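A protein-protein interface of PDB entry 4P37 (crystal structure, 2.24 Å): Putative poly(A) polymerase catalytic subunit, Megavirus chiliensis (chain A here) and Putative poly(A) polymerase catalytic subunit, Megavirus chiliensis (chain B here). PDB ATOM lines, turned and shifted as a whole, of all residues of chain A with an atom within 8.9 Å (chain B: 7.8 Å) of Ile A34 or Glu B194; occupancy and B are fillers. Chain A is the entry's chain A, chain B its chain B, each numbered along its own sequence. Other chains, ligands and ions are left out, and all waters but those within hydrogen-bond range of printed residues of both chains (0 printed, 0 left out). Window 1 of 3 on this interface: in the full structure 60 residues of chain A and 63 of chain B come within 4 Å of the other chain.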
ATOM      1  N   TYR A  23      24.380  -5.520 -24.290  1.00  0.00           N
ATOM      2  CA  TYR A  23      23.129  -5.700 -25.000  1.00  0.00           C
ATOM      3  C   TYR A  23      23.328  -6.504 -26.293  1.00  0.00           C
ATOM      4  O   TYR A  23      22.637  -7.499 -26.519  1.00  0.00           O
ATOM      5  CB  TYR A  23      22.471  -4.336 -25.309  1.00  0.00           C
ATOM      6  CG  TYR A  23      21.108  -4.521 -25.937  1.00  0.00           C
ATOM      7  CD1 TYR A  23      19.977  -4.706 -25.148  1.00  0.00           C
ATOM      8  CD2 TYR A  23      20.959  -4.616 -27.323  1.00  0.00           C
ATOM      9  CE1 TYR A  23      18.731  -4.952 -25.717  1.00  0.00           C
ATOM     10  CE2 TYR A  23      19.717  -4.887 -27.903  1.00  0.00           C
ATOM     11  CZ  TYR A  23      18.605  -5.030 -27.095  1.00  0.00           C
ATOM     12  OH  TYR A  23      17.376  -5.257 -27.656  1.00  0.00           O
ATOM     13  N   VAL A  26      24.395 -10.254 -25.870  1.00  0.00           N
ATOM     14  CA  VAL A  26      23.259 -11.081 -25.442  1.00  0.00           C
ATOM     15  C   VAL A  26      22.371 -11.381 -26.648  1.00  0.00           C
ATOM     16  O   VAL A  26      22.055 -12.546 -26.908  1.00  0.00           O
ATOM     17  CB  VAL A  26      22.459 -10.431 -24.276  1.00  0.00           C
ATOM     18  CG1 VAL A  26      21.212 -11.238 -23.928  1.00  0.00           C
ATOM     19  CG2 VAL A  26      23.325 -10.254 -23.040  1.00  0.00           C
ATOM     20  N   ARG A  27      21.998 -10.316 -27.381  1.00  0.00           N
ATOM     21  CA  ARG A  27      21.137 -10.355 -28.557  1.00  0.00           C
ATOM     22  C   ARG A  27      21.629 -11.332 -29.624  1.00  0.00           C
ATOM     23  O   ARG A  27      20.839 -12.091 -30.182  1.00  0.00           O
ATOM     24  CB  ARG A  27      20.948  -8.941 -29.130  1.00  0.00           C
ATOM     25  CG  ARG A  27      19.515  -8.451 -28.976  1.00  0.00           C
ATOM     26  CD  ARG A  27      18.811  -8.209 -30.297  1.00  0.00           C
ATOM     27  NE  ARG A  27      17.387  -7.911 -30.093  1.00  0.00           N
ATOM     28  CZ  ARG A  27      16.382  -8.413 -30.803  1.00  0.00           C
ATOM     29  NH1 ARG A  27      15.130  -8.072 -30.523  1.00  0.00           N
ATOM     30  NH2 ARG A  27      16.619  -9.258 -31.799  1.00  0.00           N
ATOM     31  N   LYS A  28      22.940 -11.341 -29.859  1.00  0.00           N
ATOM     32  CA  LYS A  28      23.590 -12.228 -30.811  1.00  0.00           C
ATOM     33  C   LYS A  28      23.617 -13.674 -30.297  1.00  0.00           C
ATOM     34  O   LYS A  28      23.355 -14.582 -31.074  1.00  0.00           O
ATOM     35  CB  LYS A  28      25.020 -11.722 -31.095  1.00  0.00           C
ATOM     36  CG  LYS A  28      25.692 -12.350 -32.311  1.00  0.00           C
ATOM     37  CD  LYS A  28      27.136 -11.875 -32.452  1.00  0.00           C
ATOM     38  CE  LYS A  28      27.820 -12.423 -33.688  1.00  0.00           C
ATOM     39  NZ  LYS A  28      28.340 -13.812 -33.501  1.00  0.00           N
ATOM     40  N   LYS A  29      23.932 -13.887 -29.004  1.00  0.00           N
ATOM     41  CA  LYS A  29      24.045 -15.227 -28.415  1.00  0.00           C
ATOM     42  C   LYS A  29      22.725 -15.908 -28.074  1.00  0.00           C
ATOM     43  O   LYS A  29      22.684 -17.139 -28.078  1.00  0.00           O
ATOM     44  CB  LYS A  29      24.951 -15.215 -27.177  1.00  0.00           C
ATOM     45  CG  LYS A  29      26.419 -14.979 -27.481  1.00  0.00           C
ATOM     46  CD  LYS A  29      27.244 -15.033 -26.223  1.00  0.00           C
ATOM     47  CE  LYS A  29      28.692 -14.732 -26.482  1.00  0.00           C
ATOM     48  NZ  LYS A  29      29.451 -14.607 -25.214  1.00  0.00           N
ATOM     49  N   LEU A  30      21.662 -15.135 -27.745  1.00  0.00           N
ATOM     50  CA  LEU A  30      20.362 -15.681 -27.324  1.00  0.00           C
ATOM     51  C   LEU A  30      19.709 -16.659 -28.309  1.00  0.00           C
ATOM     52  O   LEU A  30      19.283 -17.714 -27.839  1.00  0.00           O
ATOM     53  CB  LEU A  30      19.348 -14.592 -26.937  1.00  0.00           C
ATOM     54  CG  LEU A  30      19.220 -14.256 -25.455  1.00  0.00           C
ATOM     55  CD1 LEU A  30      18.198 -13.180 -25.249  1.00  0.00           C
ATOM     56  CD2 LEU A  30      18.828 -15.480 -24.622  1.00  0.00           C
ATOM     57  N   PRO A  31      19.601 -16.383 -29.640  1.00  0.00           N
ATOM     58  CA  PRO A  31      18.932 -17.354 -30.529  1.00  0.00           C
ATOM     59  C   PRO A  31      19.462 -18.785 -30.445  1.00  0.00           C
ATOM     60  O   PRO A  31      18.655 -19.723 -30.427  1.00  0.00           O
ATOM     61  CB  PRO A  31      19.102 -16.742 -31.921  1.00  0.00           C
ATOM     62  CG  PRO A  31      19.225 -15.278 -31.667  1.00  0.00           C
ATOM     63  CD  PRO A  31      20.011 -15.179 -30.394  1.00  0.00           C
ATOM     64  N   GLU A  32      20.790 -18.957 -30.320  1.00  0.00           N
ATOM     65  CA  GLU A  32      21.378 -20.296 -30.211  1.00  0.00           C
ATOM     66  C   GLU A  32      21.143 -20.930 -28.836  1.00  0.00           C
ATOM     67  O   GLU A  32      20.887 -22.133 -28.782  1.00  0.00           O
ATOM     68  CB  GLU A  32      22.862 -20.306 -30.613  1.00  0.00           C
ATOM     69  CG  GLU A  32      23.451 -21.696 -30.838  1.00  0.00           C
ATOM     70  CD  GLU A  32      22.734 -22.643 -31.792  1.00  0.00           C
ATOM     71  OE1 GLU A  32      22.186 -22.175 -32.817  1.00  0.00           O
ATOM     72  OE2 GLU A  32      22.746 -23.866 -31.522  1.00  0.00           O
ATOM     73  N   ILE A  33      21.205 -20.128 -27.738  1.00  0.00           N
ATOM     74  CA  ILE A  33      20.953 -20.605 -26.362  1.00  0.00           C
ATOM     75  C   ILE A  33      19.509 -21.142 -26.277  1.00  0.00           C
ATOM     76  O   ILE A  33      19.295 -22.241 -25.751  1.00  0.00           O
ATOM     77  CB  ILE A  33      21.261 -19.506 -25.282  1.00  0.00           C
ATOM     78  CG1 ILE A  33      22.775 -19.169 -25.249  1.00  0.00           C
ATOM     79  CG2 ILE A  33      20.782 -19.946 -23.887  1.00  0.00           C
ATOM     80  CD1 ILE A  33      23.155 -17.838 -24.658  1.00  0.00           C
ATOM     81  N   ILE A  34      18.538 -20.362 -26.828  1.00  0.00           N
ATOM     82  CA  ILE A  34      17.106 -20.689 -26.894  1.00  0.00           C
ATOM     83  C   ILE A  34      16.896 -22.013 -27.653  1.00  0.00           C
ATOM     84  O   ILE A  34      16.162 -22.875 -27.163  1.00  0.00           O
ATOM     85  CB  ILE A  34      16.256 -19.495 -27.453  1.00  0.00           C
ATOM     86  CG1 ILE A  34      16.297 -18.280 -26.471  1.00  0.00           C
ATOM     87  CG2 ILE A  34      14.812 -19.914 -27.779  1.00  0.00           C
ATOM     88  CD1 ILE A  34      15.669 -16.981 -26.932  1.00  0.00           C
ATOM     89  N   LYS A  35      17.592 -22.195 -28.804  1.00  0.00           N
ATOM     90  CA  LYS A  35      17.530 -23.410 -29.627  1.00  0.00           C
ATOM     91  C   LYS A  35      17.972 -24.625 -28.814  1.00  0.00           C
ATOM     92  O   LYS A  35      17.322 -25.675 -28.868  1.00  0.00           O
ATOM     93  CB  LYS A  35      18.409 -23.257 -30.888  1.00  0.00           C
ATOM     94  CG  LYS A  35      18.279 -24.426 -31.867  1.00  0.00           C
ATOM     95  CD  LYS A  35      19.185 -24.293 -33.063  1.00  0.00           C
ATOM     96  CE  LYS A  35      18.909 -25.401 -34.049  1.00  0.00           C
ATOM     97  NZ  LYS A  35      19.520 -25.130 -35.374  1.00  0.00           N
ATOM     98  N   GLN A  36      19.077 -24.474 -28.051  1.00  0.00           N
ATOM     99  CA  GLN A  36      19.626 -25.537 -27.207  1.00  0.00           C
ATOM    100  C   GLN A  36      18.704 -25.889 -26.040  1.00  0.00           C
ATOM    101  O   GLN A  36      18.563 -27.071 -25.710  1.00  0.00           O
ATOM    102  CB  GLN A  36      21.060 -25.196 -26.744  1.00  0.00           C
ATOM    103  CG  GLN A  36      22.115 -25.205 -27.869  1.00  0.00           C
ATOM    104  CD  GLN A  36      21.988 -26.386 -28.823  1.00  0.00           C
ATOM    105  OE1 GLN A  36      22.019 -27.569 -28.432  1.00  0.00           O
ATOM    106  NE2 GLN A  36      21.810 -26.084 -30.098  1.00  0.00           N
ATOM    107  N   ALA A  37      18.025 -24.876 -25.466  1.00  0.00           N
ATOM    108  CA  ALA A  37      17.057 -25.074 -24.379  1.00  0.00           C
ATOM    109  C   ALA A  37      15.855 -25.836 -24.918  1.00  0.00           C
ATOM    110  O   ALA A  37      15.372 -26.741 -24.249  1.00  0.00           O
ATOM    111  CB  ALA A  37      16.627 -23.735 -23.790  1.00  0.00           C
ATOM    112  N   ARG A  38      15.421 -25.517 -26.158  1.00  0.00           N
ATOM    113  CA  ARG A  38      14.313 -26.204 -26.846  1.00  0.00           C
ATOM    114  C   ARG A  38      14.684 -27.666 -27.162  1.00  0.00           C
ATOM    115  O   ARG A  38      13.892 -28.557 -26.863  1.00  0.00           O
ATOM    116  CB  ARG A  38      13.915 -25.459 -28.113  1.00  0.00           C
ATOM    117  CG  ARG A  38      13.136 -24.176 -27.853  1.00  0.00           C
ATOM    118  CD  ARG A  38      12.735 -23.509 -29.156  1.00  0.00           C
ATOM    119  NE  ARG A  38      11.907 -24.382 -29.992  1.00  0.00           N
ATOM    120  CZ  ARG A  38      11.386 -24.029 -31.160  1.00  0.00           C
ATOM    121  NH1 ARG A  38      11.584 -22.806 -31.640  1.00  0.00           N
ATOM    122  NH2 ARG A  38      10.654 -24.890 -31.853  1.00  0.00           N
ATOM    123  N   ILE A  39      15.913 -27.907 -27.697  1.00  0.00           N
ATOM    124  CA  ILE A  39      16.449 -29.240 -27.990  1.00  0.00           C
ATOM    125  C   ILE A  39      16.486 -30.095 -26.705  1.00  0.00           C
ATOM    126  O   ILE A  39      15.963 -31.213 -26.709  1.00  0.00           O
ATOM    127  CB  ILE A  39      17.829 -29.172 -28.725  1.00  0.00           C
ATOM    128  CG1 ILE A  39      17.653 -28.727 -30.183  1.00  0.00           C
ATOM    129  CG2 ILE A  39      18.598 -30.513 -28.667  1.00  0.00           C
ATOM    130  CD1 ILE A  39      18.897 -28.074 -30.803  1.00  0.00           C
ATOM    131  N   LYS A  40      17.061 -29.557 -25.606  1.00  0.00           N
ATOM    132  CA  LYS A  40      17.132 -30.259 -24.319  1.00  0.00           C
ATOM    133  C   LYS A  40      15.734 -30.597 -23.783  1.00  0.00           C
ATOM    134  O   LYS A  40      15.485 -31.741 -23.386  1.00  0.00           O
ATOM    135  CB  LYS A  40      17.953 -29.448 -23.293  1.00  0.00           C
ATOM    136  CG  LYS A  40      18.036 -30.077 -21.896  1.00  0.00           C
ATOM    137  CD  LYS A  40      18.841 -31.383 -21.839  1.00  0.00           C
ATOM    138  CE  LYS A  40      18.802 -31.987 -20.455  1.00  0.00           C
ATOM    139  NZ  LYS A  40      19.420 -33.336 -20.408  1.00  0.00           N
ATOM    140  N   ALA A  41      14.824 -29.602 -23.798  1.00  0.00           N
ATOM    141  CA  ALA A  41      13.439 -29.764 -23.352  1.00  0.00           C
ATOM    142  C   ALA A  41      12.754 -30.920 -24.087  1.00  0.00           C
ATOM    143  O   ALA A  41      12.106 -31.731 -23.443  1.00  0.00           O
ATOM    144  CB  ALA A  41      12.664 -28.476 -23.561  1.00  0.00           C
ATOM    145  N   LEU A  94      13.883 -30.484 -34.704  1.00  0.00           N
ATOM    146  CA  LEU A  94      12.847 -29.946 -33.815  1.00  0.00           C
ATOM    147  C   LEU A  94      11.453 -30.195 -34.369  1.00  0.00           C
ATOM    148  O   LEU A  94      11.261 -30.203 -35.594  1.00  0.00           O
ATOM    149  CB  LEU A  94      13.041 -28.434 -33.581  1.00  0.00           C
ATOM    150  CG  LEU A  94      14.180 -27.999 -32.646  1.00  0.00           C
ATOM    151  CD1 LEU A  94      14.509 -26.527 -32.843  1.00  0.00           C
ATOM    152  CD2 LEU A  94      13.824 -28.233 -31.181  1.00  0.00           C
ATOM    153  N   ILE B 182      13.820 -16.016 -16.536  1.00  0.00           N
ATOM    154  CA  ILE B 182      15.216 -16.369 -16.802  1.00  0.00           C
ATOM    155  C   ILE B 182      15.602 -17.661 -16.062  1.00  0.00           C
ATOM    156  O   ILE B 182      16.356 -18.467 -16.603  1.00  0.00           O
ATOM    157  CB  ILE B 182      16.229 -15.196 -16.503  1.00  0.00           C
ATOM    158  CG1 ILE B 182      15.926 -13.887 -17.275  1.00  0.00           C
ATOM    159  CG2 ILE B 182      17.677 -15.628 -16.736  1.00  0.00           C
ATOM    160  CD1 ILE B 182      15.716 -13.986 -18.786  1.00  0.00           C
ATOM    161  N   PRO B 185      14.652 -22.177 -17.566  1.00  0.00           N
ATOM    162  CA  PRO B 185      15.106 -22.321 -18.957  1.00  0.00           C
ATOM    163  C   PRO B 185      14.322 -23.270 -19.863  1.00  0.00           C
ATOM    164  O   PRO B 185      14.159 -22.959 -21.037  1.00  0.00           O
ATOM    165  CB  PRO B 185      16.556 -22.784 -18.806  1.00  0.00           C
ATOM    166  CG  PRO B 185      16.630 -23.375 -17.438  1.00  0.00           C
ATOM    167  CD  PRO B 185      15.739 -22.520 -16.624  1.00  0.00           C
ATOM    168  N   ALA B 188      10.437 -21.444 -20.199  1.00  0.00           N
ATOM    169  CA  ALA B 188      10.255 -20.041 -20.564  1.00  0.00           C
ATOM    170  C   ALA B 188      11.193 -19.491 -21.629  1.00  0.00           C
ATOM    171  O   ALA B 188      10.895 -18.414 -22.132  1.00  0.00           O
ATOM    172  CB  ALA B 188      10.326 -19.170 -19.312  1.00  0.00           C
ATOM    173  N   ALA B 189      12.297 -20.181 -21.974  1.00  0.00           N
ATOM    174  CA  ALA B 189      13.277 -19.653 -22.932  1.00  0.00           C
ATOM    175  C   ALA B 189      12.688 -19.214 -24.264  1.00  0.00           C
ATOM    176  O   ALA B 189      12.803 -18.031 -24.621  1.00  0.00           O
ATOM    177  CB  ALA B 189      14.423 -20.634 -23.152  1.00  0.00           C
ATOM    178  N   GLU B 190      12.009 -20.153 -24.960  1.00  0.00           N
ATOM    179  CA  GLU B 190      11.411 -19.961 -26.282  1.00  0.00           C
ATOM    180  C   GLU B 190      10.495 -18.750 -26.392  1.00  0.00           C
ATOM    181  O   GLU B 190      10.673 -17.940 -27.303  1.00  0.00           O
ATOM    182  CB  GLU B 190      10.680 -21.236 -26.741  1.00  0.00           C
ATOM    183  CG  GLU B 190      10.147 -21.163 -28.167  1.00  0.00           C
ATOM    184  CD  GLU B 190       9.169 -22.260 -28.534  1.00  0.00           C
ATOM    185  OE1 GLU B 190       8.127 -21.938 -29.148  1.00  0.00           O
ATOM    186  OE2 GLU B 190       9.437 -23.438 -28.201  1.00  0.00           O
ATOM    187  N   GLN B 191       9.527 -18.627 -25.481  1.00  0.00           N
ATOM    188  CA  GLN B 191       8.542 -17.551 -25.547  1.00  0.00           C
ATOM    189  C   GLN B 191       8.855 -16.295 -24.725  1.00  0.00           C
ATOM    190  O   GLN B 191       8.290 -15.235 -25.034  1.00  0.00           O
ATOM    191  CB  GLN B 191       7.148 -18.089 -25.147  1.00  0.00           C
ATOM    192  CG  GLN B 191       6.584 -19.178 -26.070  1.00  0.00           C
ATOM    193  CD  GLN B 191       6.003 -18.618 -27.342  1.00  0.00           C
ATOM    194  OE1 GLN B 191       4.912 -18.039 -27.353  1.00  0.00           O
ATOM    195  NE2 GLN B 191       6.712 -18.793 -28.444  1.00  0.00           N
ATOM    196  N   ARG B 192       9.708 -16.395 -23.669  1.00  0.00           N
ATOM    197  CA  ARG B 192       9.885 -15.251 -22.779  1.00  0.00           C
ATOM    198  C   ARG B 192      11.266 -14.602 -22.671  1.00  0.00           C
ATOM    199  O   ARG B 192      11.309 -13.418 -22.339  1.00  0.00           O
ATOM    200  CB  ARG B 192       9.424 -15.607 -21.356  1.00  0.00           C
ATOM    201  CG  ARG B 192       8.011 -16.152 -21.261  1.00  0.00           C
ATOM    202  CD  ARG B 192       7.392 -15.679 -19.993  1.00  0.00           C
ATOM    203  NE  ARG B 192       5.984 -15.338 -20.152  1.00  0.00           N
ATOM    204  CZ  ARG B 192       5.527 -14.105 -20.343  1.00  0.00           C
ATOM    205  NH1 ARG B 192       6.369 -13.094 -20.503  1.00  0.00           N
ATOM    206  NH2 ARG B 192       4.226 -13.888 -20.463  1.00  0.00           N
ATOM    207  N   TRP B 193      12.372 -15.330 -22.907  1.00  0.00           N
ATOM    208  CA  TRP B 193      13.739 -14.825 -22.681  1.00  0.00           C
ATOM    209  C   TRP B 193      14.145 -13.536 -23.438  1.00  0.00           C
ATOM    210  O   TRP B 193      14.741 -12.653 -22.810  1.00  0.00           O
ATOM    211  CB  TRP B 193      14.775 -15.918 -22.912  1.00  0.00           C
ATOM    212  CG  TRP B 193      14.933 -16.827 -21.723  1.00  0.00           C
ATOM    213  CD1 TRP B 193      14.019 -17.057 -20.734  1.00  0.00           C
ATOM    214  CD2 TRP B 193      16.068 -17.648 -21.421  1.00  0.00           C
ATOM    215  NE1 TRP B 193      14.506 -17.986 -19.845  1.00  0.00           N
ATOM    216  CE2 TRP B 193      15.765 -18.364 -20.240  1.00  0.00           C
ATOM    217  CE3 TRP B 193      17.309 -17.859 -22.039  1.00  0.00           C
ATOM    218  CZ2 TRP B 193      16.675 -19.241 -19.645  1.00  0.00           C
ATOM    219  CZ3 TRP B 193      18.188 -18.774 -21.476  1.00  0.00           C
ATOM    220  CH2 TRP B 193      17.874 -19.444 -20.291  1.00  0.00           C
ATOM    221  N   GLU B 194      13.838 -13.423 -24.748  1.00  0.00           N
ATOM    222  CA  GLU B 194      14.177 -12.231 -25.535  1.00  0.00           C
ATOM    223  C   GLU B 194      13.468 -10.987 -25.011  1.00  0.00           C
ATOM    224  O   GLU B 194      14.108  -9.955 -24.825  1.00  0.00           O
ATOM    225  CB  GLU B 194      13.883 -12.450 -27.023  1.00  0.00           C
ATOM    226  CG  GLU B 194      14.880 -13.386 -27.686  1.00  0.00           C
ATOM    227  CD  GLU B 194      14.535 -13.853 -29.090  1.00  0.00           C
ATOM    228  OE1 GLU B 194      13.433 -14.418 -29.279  1.00  0.00           O
ATOM    229  OE2 GLU B 194      15.400 -13.715 -29.986  1.00  0.00           O
ATOM    230  N   LYS B 195      12.164 -11.107 -24.727  1.00  0.00           N
ATOM    231  CA  LYS B 195      11.332 -10.035 -24.183  1.00  0.00           C
ATOM    232  C   LYS B 195      11.742  -9.702 -22.732  1.00  0.00           C
ATOM    233  O   LYS B 195      11.802  -8.519 -22.390  1.00  0.00           O
ATOM    234  CB  LYS B 195       9.850 -10.433 -24.268  1.00  0.00           C
ATOM    235  CG  LYS B 195       8.857  -9.262 -24.185  1.00  0.00           C
ATOM    236  CD  LYS B 195       7.417  -9.786 -24.178  1.00  0.00           C
ATOM    237  CE  LYS B 195       6.372  -8.702 -24.144  1.00  0.00           C
ATOM    238  NZ  LYS B 195       5.002  -9.270 -24.018  1.00  0.00           N
ATOM    239  N   ALA B 196      12.028 -10.735 -21.896  1.00  0.00           N
ATOM    240  CA  ALA B 196      12.462 -10.572 -20.504  1.00  0.00           C
ATOM    241  C   ALA B 196      13.781  -9.785 -20.440  1.00  0.00           C
ATOM    242  O   ALA B 196      13.898  -8.862 -19.618  1.00  0.00           O
ATOM    243  CB  ALA B 196      12.629 -11.929 -19.828  1.00  0.00           C
ATOM    244  N   PHE B 197      14.755 -10.116 -21.336  1.00  0.00           N
ATOM    245  CA  PHE B 197      16.023  -9.399 -21.392  1.00  0.00           C
ATOM    246  C   PHE B 197      15.819  -7.942 -21.770  1.00  0.00           C
ATOM    247  O   PHE B 197      16.386  -7.072 -21.120  1.00  0.00           O
ATOM    248  CB  PHE B 197      17.051 -10.078 -22.316  1.00  0.00           C
ATOM    249  CG  PHE B 197      18.328  -9.283 -22.431  1.00  0.00           C
ATOM    250  CD1 PHE B 197      19.187  -9.146 -21.340  1.00  0.00           C
ATOM    251  CD2 PHE B 197      18.648  -8.619 -23.611  1.00  0.00           C
ATOM    252  CE1 PHE B 197      20.362  -8.397 -21.445  1.00  0.00           C
ATOM    253  CE2 PHE B 197      19.820  -7.869 -23.715  1.00  0.00           C
ATOM    254  CZ  PHE B 197      20.663  -7.750 -22.627  1.00  0.00           C
ATOM    255  N   ASP B 198      15.001  -7.681 -22.789  1.00  0.00           N
ATOM    256  CA  ASP B 198      14.687  -6.334 -23.260  1.00  0.00           C
ATOM    257  C   ASP B 198      14.113  -5.483 -22.155  1.00  0.00           C
ATOM    258  O   ASP B 198      14.550  -4.349 -21.974  1.00  0.00           O
ATOM    259  CB  ASP B 198      13.697  -6.385 -24.441  1.00  0.00           C
ATOM    260  CG  ASP B 198      14.321  -6.596 -25.812  1.00  0.00           C
ATOM    261  OD1 ASP B 198      15.579  -6.664 -25.900  1.00  0.00           O
ATOM    262  OD2 ASP B 198      13.555  -6.691 -26.796  1.00  0.00           O
ATOM    263  N   ARG B 199      13.135  -6.030 -21.410  1.00  0.00           N
ATOM    264  CA  ARG B 199      12.486  -5.339 -20.293  1.00  0.00           C
ATOM    265  C   ARG B 199      13.452  -5.098 -19.116  1.00  0.00           C
ATOM    266  O   ARG B 199      13.500  -3.988 -18.590  1.00  0.00           O
ATOM    267  CB  ARG B 199      11.200  -6.071 -19.852  1.00  0.00           C
ATOM    268  CG  ARG B 199      10.125  -6.237 -20.951  1.00  0.00           C
ATOM    269  CD  ARG B 199       9.208  -5.035 -21.064  1.00  0.00           C
ATOM    270  NE  ARG B 199       8.017  -5.279 -21.889  1.00  0.00           N
ATOM    271  CZ  ARG B 199       6.831  -5.673 -21.419  1.00  0.00           C
ATOM    272  NH1 ARG B 199       6.667  -5.918 -20.124  1.00  0.00           N
ATOM    273  NH2 ARG B 199       5.807  -5.844 -22.246  1.00  0.00           N
ATOM    274  N   MET B 200      14.235  -6.123 -18.738  1.00  0.00           N
ATOM    275  CA  MET B 200      15.231  -6.075 -17.657  1.00  0.00           C
ATOM    276  C   MET B 200      16.271  -5.000 -17.936  1.00  0.00           C
ATOM    277  O   MET B 200      16.574  -4.205 -17.043  1.00  0.00           O
ATOM    278  CB  MET B 200      15.956  -7.419 -17.534  1.00  0.00           C
ATOM    279  CG  MET B 200      15.279  -8.398 -16.632  1.00  0.00           C
ATOM    280  SD  MET B 200      16.417  -9.937 -16.208  1.00  0.00           S
ATOM    281  CE  MET B 200      18.044  -8.992 -15.477  1.00  0.00           C
ATOM    282  N   PHE B 425      21.846 -16.440 -18.513  1.00  0.00           N
ATOM    283  CA  PHE B 425      21.086 -17.256 -19.481  1.00  0.00           C
ATOM    284  C   PHE B 425      21.580 -18.718 -19.580  1.00  0.00           C
ATOM    285  O   PHE B 425      21.734 -19.268 -20.672  1.00  0.00           O
ATOM    286  CB  PHE B 425      21.038 -16.567 -20.860  1.00  0.00           C
ATOM    287  CG  PHE B 425      20.466 -15.170 -20.783  1.00  0.00           C
ATOM    288  CD1 PHE B 425      19.089 -14.963 -20.767  1.00  0.00           C
ATOM    289  CD2 PHE B 425      21.303 -14.065 -20.689  1.00  0.00           C
ATOM    290  CE1 PHE B 425      18.559 -13.676 -20.656  1.00  0.00           C
ATOM    291  CE2 PHE B 425      20.774 -12.780 -20.567  1.00  0.00           C
ATOM    292  CZ  PHE B 425      19.403 -12.596 -20.533  1.00  0.00           C
ATOM    293  N   ILE B 427      21.291 -22.754 -19.276  1.00  0.00           N
ATOM    294  CA  ILE B 427      20.194 -23.667 -19.583  1.00  0.00           C
ATOM    295  C   ILE B 427      20.278 -24.967 -18.782  1.00  0.00           C
ATOM    296  O   ILE B 427      19.265 -25.650 -18.668  1.00  0.00           O
ATOM    297  CB  ILE B 427      20.015 -23.898 -21.098  1.00  0.00           C
ATOM    298  CG1 ILE B 427      21.223 -24.581 -21.752  1.00  0.00           C
ATOM    299  CG2 ILE B 427      19.673 -22.576 -21.798  1.00  0.00           C
ATOM    300  CD1 ILE B 427      20.909 -25.260 -23.084  1.00  0.00           C
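Of the 17 printed residues of chain B, 9 touch a printed residue of chain A. Hydrophobic or aromatic side chains of chain B that line the printed part of chain A: Ala B189, Trp B193, Phe B197, Phe B425 and Ile B427. Of the 18 printed residues of chain A, 8 touch a printed residue of chain B. Hydrophobic or aromatic side chains of chain A that line the printed part of chain B: Tyr A23, Val A26, Leu A30, Ile A33, Ile A34 and Ala A37.
The side-chain carboxylate (OE2) of Glu A32 lies within hydrogen-bond range of the side-chain amide nitrogen (NE2) of Gln A36 (2.8 Å).
The side-chain carboxylate of Asp B198 is in hydrogen-bond range of the side-chain hydroxyl of Tyr A23. The guanidinium group (NE) of Arg A38 is in salt-bridge range of the side-chain carboxylate (OE2) of Glu B190 (3.2 Å).
Among the printed residues, pairs that only touch across the chains: Ile A33 with Phe B425, Tyr A23 with Phe B197, Ile A33 with Ile B427, Val A26 with Phe B197, Gln A36 with Ile B427, Ile A34 with Glu B190, Val A26 with Phe B425, Ile A33 with Trp B193, Ile A34 with Glu B194, Ala A37 with Ile B427, Ala A37 with Pro B185, Leu A30 with Trp B193, Ile A34 with Ala B189, Ala A37 with Ala B189 and Leu A30 with Phe B425.
Of the printed residues of chain B, Ile A33 touches Trp B193 (3.7 Å), Phe B425 (3.4 Å) and Ile B427 (3.5 Å). Of the printed residues of chain B, Gln A36 touches Ile B427 (3.7 Å). Of the printed residues of chain B, Ala A37 touches Pro B185, Ala B189 and Ile B427. Printed residues of chain A within 4 Å of Ala B189: Ile A34 and Ala A37. Glu B194 touches just one residue of chain A: Ile A34. Of the printed residues of chain A, Asp B198 touches Tyr A23. The nearest residue of chain B that does not touch Ile A34 is Trp B193 (4.3 Å).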
